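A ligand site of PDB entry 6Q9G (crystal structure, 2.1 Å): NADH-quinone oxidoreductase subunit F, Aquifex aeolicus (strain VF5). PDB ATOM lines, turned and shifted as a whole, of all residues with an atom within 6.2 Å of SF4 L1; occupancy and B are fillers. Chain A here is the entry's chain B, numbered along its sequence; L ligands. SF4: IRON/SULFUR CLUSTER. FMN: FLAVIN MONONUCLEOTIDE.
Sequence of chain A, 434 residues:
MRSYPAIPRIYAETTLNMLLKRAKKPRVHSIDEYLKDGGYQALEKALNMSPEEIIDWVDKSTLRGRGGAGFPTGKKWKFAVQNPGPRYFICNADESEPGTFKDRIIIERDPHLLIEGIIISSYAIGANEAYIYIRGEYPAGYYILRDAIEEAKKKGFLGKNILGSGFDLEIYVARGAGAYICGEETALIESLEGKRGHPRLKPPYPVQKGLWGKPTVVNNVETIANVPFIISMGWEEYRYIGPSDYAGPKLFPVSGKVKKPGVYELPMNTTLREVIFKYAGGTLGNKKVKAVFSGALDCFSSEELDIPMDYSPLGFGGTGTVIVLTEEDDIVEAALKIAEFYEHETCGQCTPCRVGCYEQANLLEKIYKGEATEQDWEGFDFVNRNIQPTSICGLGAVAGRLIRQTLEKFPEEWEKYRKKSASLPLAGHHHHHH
N of Cys 347 lies close to S4 of SF4 L1 (3.7 Å). FE1 of SF4 L1 is bound by SG of Cys 347 (2.3 Å). S3 of SF4 L1 sits close to N of Cys 350 (3.2 Å). An iron atom (FE4) of SF4 L1 is bound by the side-chain sulfur (SG) of Cys 350 (2.3 Å). FE3 of SF4 L1 is bound by SG of Cys 393 (2.3 Å). An iron atom (FE2) of SF4 L1 is bound by the side-chain sulfur of Cys 353, 2.3 Å away. N of Gln 349 lies close to S3 of SF4 L1. The side-chain amide nitrogen (NE2) of Gln 349 sits close to a sulfur (S2) of SF4 L1, at 3.6 Å. The backbone NH of Gly 396 sits close to a sulfur (S1) of SF4 L1. S3 of SF4 L1 sits close to N of Gly 348, 3.6 Å away. S3 of SF4 L1 lies close to OG1 of Thr 346 (3.8 Å).
The side-chain sulfur (SG) of Cys 347 sits close to the side-chain amide nitrogen (NE2) of Gln 349, at 3.6 Å. SG of Cys 350 lies close to N of Ile 392, 3.7 Å away. SG of Cys 353 sits close to OG1 of Thr 346, 3.2 Å away. The backbone carbonyl oxygen (O) of Cys 353 lies close to the side-chain sulfur (SG) of Cys 357. N of Cys 353 lies within hydrogen-bond range of O of Ile 387, 3.4 Å away. The side-chain amide nitrogen (NE2) of Gln 349 sits at hydrogen-bond distance from the backbone carbonyl oxygen (O) of Pro 199, 2.9 Å away. OG1 of Thr 346 sits at hydrogen-bond distance from N of Gly 348. The guanidinium group (NH1) of Arg 354 sits at hydrogen-bond distance from the backbone carbonyl oxygen (O) of Gly 348, at 2.8 Å.
CD1 of Ile 181 touches S4 of SF4 L1, 3.6 Å away. Pro 199 touches SF4 L1. Ser 391 touches SF4 L1. Ile 392 touches SF4 L1. Leu 395 touches SF4 L1 (CB to S4, 3.7 Å). Hydrophobic or aromatic side chains that line SF4 L1: Ile 181, Pro 199, Ile 392 and Leu 395. Of the 22 residues printed, 13 come within 4 Å of SF4 L1. Along chain A the residues within 4 Å of SF4 L1 span positions 181 to 396. The nearest printed residue that does not touch SF4 L1 is Arg 354 (4.7 Å).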
ATOM      1  N   ILE A 181      20.828  23.680  -6.028  1.00  0.00           N
ATOM      2  CA  ILE A 181      20.084  24.910  -6.454  1.00  0.00           C
ATOM      3  C   ILE A 181      20.023  24.973  -7.983  1.00  0.00           C
ATOM      4  O   ILE A 181      19.069  25.562  -8.476  1.00  0.00           O
ATOM      5  CB  ILE A 181      20.708  26.191  -5.860  1.00  0.00           C
ATOM      6  CG1 ILE A 181      19.789  27.402  -6.050  1.00  0.00           C
ATOM      7  CG2 ILE A 181      22.088  26.470  -6.439  1.00  0.00           C
ATOM      8  CD1 ILE A 181      18.394  27.186  -5.526  1.00  0.00           C
ATOM      9  N   HIS A 198      22.450  30.945  -9.638  1.00  0.00           N
ATOM     10  CA  HIS A 198      21.653  31.916  -8.847  1.00  0.00           C
ATOM     11  C   HIS A 198      20.277  32.021  -9.476  1.00  0.00           C
ATOM     12  O   HIS A 198      20.152  32.503 -10.598  1.00  0.00           O
ATOM     13  CB  HIS A 198      22.364  33.272  -8.765  1.00  0.00           C
ATOM     14  CG  HIS A 198      23.550  33.275  -7.864  1.00  0.00           C
ATOM     15  ND1 HIS A 198      24.548  34.206  -7.961  1.00  0.00           N
ATOM     16  CD2 HIS A 198      23.909  32.448  -6.857  1.00  0.00           C
ATOM     17  CE1 HIS A 198      25.459  33.969  -7.044  1.00  0.00           C
ATOM     18  NE2 HIS A 198      25.096  32.908  -6.350  1.00  0.00           N
ATOM     19  N   PRO A 199      19.209  31.549  -8.791  1.00  0.00           N
ATOM     20  CA  PRO A 199      17.843  31.744  -9.264  1.00  0.00           C
ATOM     21  C   PRO A 199      17.542  33.205  -9.625  1.00  0.00           C
ATOM     22  O   PRO A 199      18.131  34.120  -9.057  1.00  0.00           O
ATOM     23  CB  PRO A 199      16.988  31.280  -8.078  1.00  0.00           C
ATOM     24  CG  PRO A 199      17.849  30.271  -7.360  1.00  0.00           C
ATOM     25  CD  PRO A 199      19.265  30.777  -7.537  1.00  0.00           C
ATOM     26  N   GLU A 345      23.144  24.007   0.764  1.00  0.00           N
ATOM     27  CA  GLU A 345      22.626  24.243  -0.624  1.00  0.00           C
ATOM     28  C   GLU A 345      22.096  25.674  -0.878  1.00  0.00           C
ATOM     29  O   GLU A 345      21.974  26.030  -2.071  1.00  0.00           O
ATOM     30  CB  GLU A 345      21.568  23.211  -0.979  1.00  0.00           C
ATOM     31  CG  GLU A 345      22.103  21.790  -1.019  1.00  0.00           C
ATOM     32  CD  GLU A 345      23.341  21.509  -1.862  1.00  0.00           C
ATOM     33  OE1 GLU A 345      23.643  22.282  -2.784  1.00  0.00           O
ATOM     34  OE2 GLU A 345      24.003  20.477  -1.595  1.00  0.00           O
ATOM     35  N   THR A 346      21.757  26.462   0.138  1.00  0.00           N
ATOM     36  CA  THR A 346      21.328  27.875  -0.088  1.00  0.00           C
ATOM     37  C   THR A 346      22.401  28.585  -0.929  1.00  0.00           C
ATOM     38  O   THR A 346      23.578  28.437  -0.607  1.00  0.00           O
ATOM     39  CB  THR A 346      21.053  28.636   1.222  1.00  0.00           C
ATOM     40  OG1 THR A 346      20.804  29.991   0.853  1.00  0.00           O
ATOM     41  CG2 THR A 346      22.186  28.573   2.222  1.00  0.00           C
ATOM     42  N   CYS A 347      21.995  29.327  -1.957  1.00  0.00           N
ATOM     43  CA  CYS A 347      22.922  30.100  -2.842  1.00  0.00           C
ATOM     44  C   CYS A 347      23.327  31.431  -2.172  1.00  0.00           C
ATOM     45  O   CYS A 347      24.324  32.012  -2.608  1.00  0.00           O
ATOM     46  CB  CYS A 347      22.316  30.293  -4.225  1.00  0.00           C
ATOM     47  SG  CYS A 347      21.110  31.641  -4.354  1.00  0.00           S
ATOM     48  N   GLY A 348      22.575  31.904  -1.180  1.00  0.00           N
ATOM     49  CA  GLY A 348      22.965  33.054  -0.342  1.00  0.00           C
ATOM     50  C   GLY A 348      22.501  34.420  -0.853  1.00  0.00           C
ATOM     51  O   GLY A 348      22.705  35.389  -0.138  1.00  0.00           O
ATOM     52  N   GLN A 349      21.873  34.497  -2.036  1.00  0.00           N
ATOM     53  CA  GLN A 349      21.373  35.767  -2.647  1.00  0.00           C
ATOM     54  C   GLN A 349      20.428  36.503  -1.689  1.00  0.00           C
ATOM     55  O   GLN A 349      20.519  37.749  -1.608  1.00  0.00           O
ATOM     56  CB  GLN A 349      20.554  35.496  -3.920  1.00  0.00           C
ATOM     57  CG  GLN A 349      21.351  35.378  -5.204  1.00  0.00           C
ATOM     58  CD  GLN A 349      20.398  35.340  -6.374  1.00  0.00           C
ATOM     59  OE1 GLN A 349      20.142  36.373  -6.992  1.00  0.00           O
ATOM     60  NE2 GLN A 349      19.823  34.164  -6.646  1.00  0.00           N
ATOM     61  N   CYS A 350      19.527  35.770  -1.040  1.00  0.00           N
ATOM     62  CA  CYS A 350      18.459  36.299  -0.150  1.00  0.00           C
ATOM     63  C   CYS A 350      18.907  36.160   1.301  1.00  0.00           C
ATOM     64  O   CYS A 350      19.304  35.063   1.688  1.00  0.00           O
ATOM     65  CB  CYS A 350      17.156  35.530  -0.336  1.00  0.00           C
ATOM     66  SG  CYS A 350      16.743  35.261  -2.067  1.00  0.00           S
ATOM     67  N   THR A 351      18.821  37.245   2.074  1.00  0.00           N
ATOM     68  CA  THR A 351      19.443  37.336   3.429  1.00  0.00           C
ATOM     69  C   THR A 351      18.816  36.318   4.374  1.00  0.00           C
ATOM     70  O   THR A 351      19.544  35.541   4.991  1.00  0.00           O
ATOM     71  CB  THR A 351      19.426  38.791   3.933  1.00  0.00           C
ATOM     72  OG1 THR A 351      20.454  39.467   3.214  1.00  0.00           O
ATOM     73  CG2 THR A 351      19.654  38.884   5.425  1.00  0.00           C
ATOM     74  N   CYS A 353      17.150  33.536   3.812  1.00  0.00           N
ATOM     75  CA  CYS A 353      17.535  32.186   3.349  1.00  0.00           C
ATOM     76  C   CYS A 353      18.999  31.945   3.746  1.00  0.00           C
ATOM     77  O   CYS A 353      19.270  30.907   4.421  1.00  0.00           O
ATOM     78  CB  CYS A 353      17.354  32.012   1.852  1.00  0.00           C
ATOM     79  SG  CYS A 353      17.659  30.309   1.287  1.00  0.00           S
ATOM     80  N   ARG A 354      19.889  32.866   3.389  1.00  0.00           N
ATOM     81  CA  ARG A 354      21.357  32.742   3.625  1.00  0.00           C
ATOM     82  C   ARG A 354      21.612  32.465   5.112  1.00  0.00           C
ATOM     83  O   ARG A 354      22.227  31.439   5.407  1.00  0.00           O
ATOM     84  CB  ARG A 354      22.089  33.990   3.145  1.00  0.00           C
ATOM     85  CG  ARG A 354      23.603  33.966   3.363  1.00  0.00           C
ATOM     86  CD  ARG A 354      24.301  35.184   2.791  1.00  0.00           C
ATOM     87  NE  ARG A 354      24.003  36.434   3.501  1.00  0.00           N
ATOM     88  CZ  ARG A 354      23.182  37.398   3.078  1.00  0.00           C
ATOM     89  NH1 ARG A 354      22.537  37.296   1.932  1.00  0.00           N
ATOM     90  NH2 ARG A 354      23.022  38.481   3.825  1.00  0.00           N
ATOM     91  N   CYS A 357      19.054  29.249   6.810  1.00  0.00           N
ATOM     92  CA  CYS A 357      19.509  27.858   6.513  1.00  0.00           C
ATOM     93  C   CYS A 357      20.729  27.532   7.400  1.00  0.00           C
ATOM     94  O   CYS A 357      20.732  26.449   8.016  1.00  0.00           O
ATOM     95  CB  CYS A 357      19.795  27.660   5.034  1.00  0.00           C
ATOM     96  SG  CYS A 357      18.289  27.691   4.030  1.00  0.00           S
ATOM     97  N   ILE A 387      12.860  31.770   7.401  1.00  0.00           N
ATOM     98  CA  ILE A 387      13.805  31.539   6.273  1.00  0.00           C
ATOM     99  C   ILE A 387      13.168  32.092   4.984  1.00  0.00           C
ATOM    100  O   ILE A 387      13.912  32.664   4.154  1.00  0.00           O
ATOM    101  CB  ILE A 387      14.200  30.056   6.154  1.00  0.00           C
ATOM    102  CG1 ILE A 387      14.807  29.551   7.474  1.00  0.00           C
ATOM    103  CG2 ILE A 387      15.168  29.860   5.002  1.00  0.00           C
ATOM    104  CD1 ILE A 387      15.006  28.062   7.563  1.00  0.00           C
ATOM    105  N   THR A 390      11.272  37.296   1.800  1.00  0.00           N
ATOM    106  CA  THR A 390      12.026  37.916   0.655  1.00  0.00           C
ATOM    107  C   THR A 390      12.610  36.873  -0.321  1.00  0.00           C
ATOM    108  O   THR A 390      13.242  37.290  -1.303  1.00  0.00           O
ATOM    109  CB  THR A 390      13.123  38.867   1.136  1.00  0.00           C
ATOM    110  OG1 THR A 390      14.283  38.120   1.518  1.00  0.00           O
ATOM    111  CG2 THR A 390      12.680  39.750   2.285  1.00  0.00           C
ATOM    112  N   SER A 391      12.417  35.566  -0.072  1.00  0.00           N
ATOM    113  CA  SER A 391      12.975  34.475  -0.912  1.00  0.00           C
ATOM    114  C   SER A 391      12.511  34.646  -2.367  1.00  0.00           C
ATOM    115  O   SER A 391      11.338  34.980  -2.565  1.00  0.00           O
ATOM    116  CB  SER A 391      12.588  33.121  -0.375  1.00  0.00           C
ATOM    117  OG  SER A 391      11.173  32.980  -0.305  1.00  0.00           O
ATOM    118  N   ILE A 392      13.410  34.413  -3.329  1.00  0.00           N
ATOM    119  CA  ILE A 392      13.104  34.499  -4.787  1.00  0.00           C
ATOM    120  C   ILE A 392      13.060  33.104  -5.397  1.00  0.00           C
ATOM    121  O   ILE A 392      12.882  33.030  -6.623  1.00  0.00           O
ATOM    122  CB  ILE A 392      14.052  35.473  -5.504  1.00  0.00           C
ATOM    123  CG1 ILE A 392      15.509  35.017  -5.536  1.00  0.00           C
ATOM    124  CG2 ILE A 392      13.933  36.871  -4.896  1.00  0.00           C
ATOM    125  CD1 ILE A 392      16.418  35.935  -6.338  1.00  0.00           C
ATOM    126  N   CYS A 393      13.182  32.020  -4.600  1.00  0.00           N
ATOM    127  CA  CYS A 393      12.986  30.632  -5.112  1.00  0.00           C
ATOM    128  C   CYS A 393      12.431  29.715  -4.014  1.00  0.00           C
ATOM    129  O   CYS A 393      12.338  30.128  -2.834  1.00  0.00           O
ATOM    130  CB  CYS A 393      14.256  30.074  -5.754  1.00  0.00           C
ATOM    131  SG  CYS A 393      15.324  29.115  -4.651  1.00  0.00           S
ATOM    132  N   GLY A 394      12.041  28.511  -4.421  1.00  0.00           N
ATOM    133  CA  GLY A 394      11.331  27.543  -3.576  1.00  0.00           C
ATOM    134  C   GLY A 394      12.181  27.004  -2.441  1.00  0.00           C
ATOM    135  O   GLY A 394      11.588  26.478  -1.494  1.00  0.00           O
ATOM    136  N   LEU A 395      13.501  27.126  -2.502  1.00  0.00           N
ATOM    137  CA  LEU A 395      14.414  26.595  -1.456  1.00  0.00           C
ATOM    138  C   LEU A 395      14.158  27.341  -0.130  1.00  0.00           C
ATOM    139  O   LEU A 395      13.822  26.684   0.867  1.00  0.00           O
ATOM    140  CB  LEU A 395      15.872  26.727  -1.914  1.00  0.00           C
ATOM    141  CG  LEU A 395      16.885  25.946  -1.079  1.00  0.00           C
ATOM    142  CD1 LEU A 395      18.095  25.560  -1.920  1.00  0.00           C
ATOM    143  CD2 LEU A 395      17.300  26.730   0.154  1.00  0.00           C
ATOM    144  N   GLY A 396      14.272  28.658  -0.146  1.00  0.00           N
ATOM    145  CA  GLY A 396      13.971  29.528   1.009  1.00  0.00           C
ATOM    146  C   GLY A 396      12.535  29.341   1.468  1.00  0.00           C
ATOM    147  O   GLY A 396      12.305  29.288   2.698  1.00  0.00           O
ATOM    148  N   ALA A 397      11.603  29.186   0.520  1.00  0.00           N
ATOM    149  CA  ALA A 397      10.168  28.983   0.801  1.00  0.00           C
ATOM    150  C   ALA A 397       9.935  27.713   1.636  1.00  0.00           C
ATOM    151  O   ALA A 397       8.926  27.672   2.367  1.00  0.00           O
ATOM    152  CB  ALA A 397       9.370  28.962  -0.487  1.00  0.00           C
HETATM  153 FE1  SF4 L   1      19.181  31.404  -3.184  1.00  0.00          FE
HETATM  154 FE2  SF4 L   1      17.710  30.818  -0.952  1.00  0.00          FE
HETATM  155 FE3  SF4 L   1      16.626  30.557  -3.435  1.00  0.00          FE
HETATM  156 FE4  SF4 L   1      17.164  33.043  -2.395  1.00  0.00          FE
HETATM  157  S1  SF4 L   1      15.638  31.508  -1.605  1.00  0.00           S
HETATM  158  S2  SF4 L   1      17.604  32.324  -4.526  1.00  0.00           S
HETATM  159  S3  SF4 L   1      19.075  32.629  -1.252  1.00  0.00           S
HETATM  160  S4  SF4 L   1      18.363  29.359  -2.596  1.00  0.00           S
HETATM  161  N1  FMN L   2      12.994  20.018 -10.961  1.00  0.00           N
HETATM  162  C2  FMN L   2      13.578  18.946 -11.561  1.00  0.00           C
HETATM  163  O2  FMN L   2      13.064  18.387 -12.527  1.00  0.00           O
HETATM  164  N3  FMN L   2      14.806  18.500 -11.123  1.00  0.00           N
HETATM  165  C4  FMN L   2      15.558  19.055 -10.107  1.00  0.00           C
HETATM  166  O4  FMN L   2      16.610  18.534  -9.770  1.00  0.00           O
HETATM  167  C4A FMN L   2      14.943  20.237  -9.495  1.00  0.00           C
HETATM  168  N5  FMN L   2      15.609  20.873  -8.571  1.00  0.00           N
HETATM  169  C5A FMN L   2      15.000  21.984  -7.983  1.00  0.00           C
HETATM  170  C6  FMN L   2      15.673  22.662  -6.959  1.00  0.00           C
HETATM  171  C7  FMN L   2      15.074  23.730  -6.291  1.00  0.00           C
HETATM  172  C7M FMN L   2      15.830  24.434  -5.188  1.00  0.00           C
HETATM  173  C8  FMN L   2      13.786  24.141  -6.656  1.00  0.00           C
HETATM  174  C8M FMN L   2      13.069  25.239  -5.899  1.00  0.00           C
HETATM  175  C9  FMN L   2      13.128  23.500  -7.704  1.00  0.00           C
HETATM  176  C9A FMN L   2      13.715  22.420  -8.368  1.00  0.00           C
HETATM  177  N10 FMN L   2      13.056  21.714  -9.410  1.00  0.00           N
HETATM  178  C10 FMN L   2      13.649  20.618  -9.977  1.00  0.00           C
HETATM  179  C1' FMN L   2      11.787  22.168  -9.975  1.00  0.00           C
HETATM  180  C2' FMN L   2      12.001  23.060 -11.191  1.00  0.00           C
HETATM  181  O2' FMN L   2      12.224  24.411 -10.763  1.00  0.00           O
HETATM  182  C3' FMN L   2      10.821  23.007 -12.149  1.00  0.00           C
HETATM  183  O3' FMN L   2       9.602  23.171 -11.430  1.00  0.00           O
HETATM  184  C4' FMN L   2      10.695  21.725 -12.973  1.00  0.00           C
HETATM  185  O4' FMN L   2      11.980  21.254 -13.401  1.00  0.00           O
HETATM  186  C5' FMN L   2       9.784  21.938 -14.168  1.00  0.00           C
HETATM  187  O5' FMN L   2       9.458  20.659 -14.743  1.00  0.00           O
HETATM  188  P   FMN L   2       8.074  19.881 -14.481  1.00  0.00           P
HETATM  189  O1P FMN L   2       7.957  19.281 -13.094  1.00  0.00           O
HETATM  190  O2P FMN L   2       6.955  20.875 -14.770  1.00  0.00           O
HETATM  191  O3P FMN L   2       8.063  18.840 -15.599  1.00  0.00           O
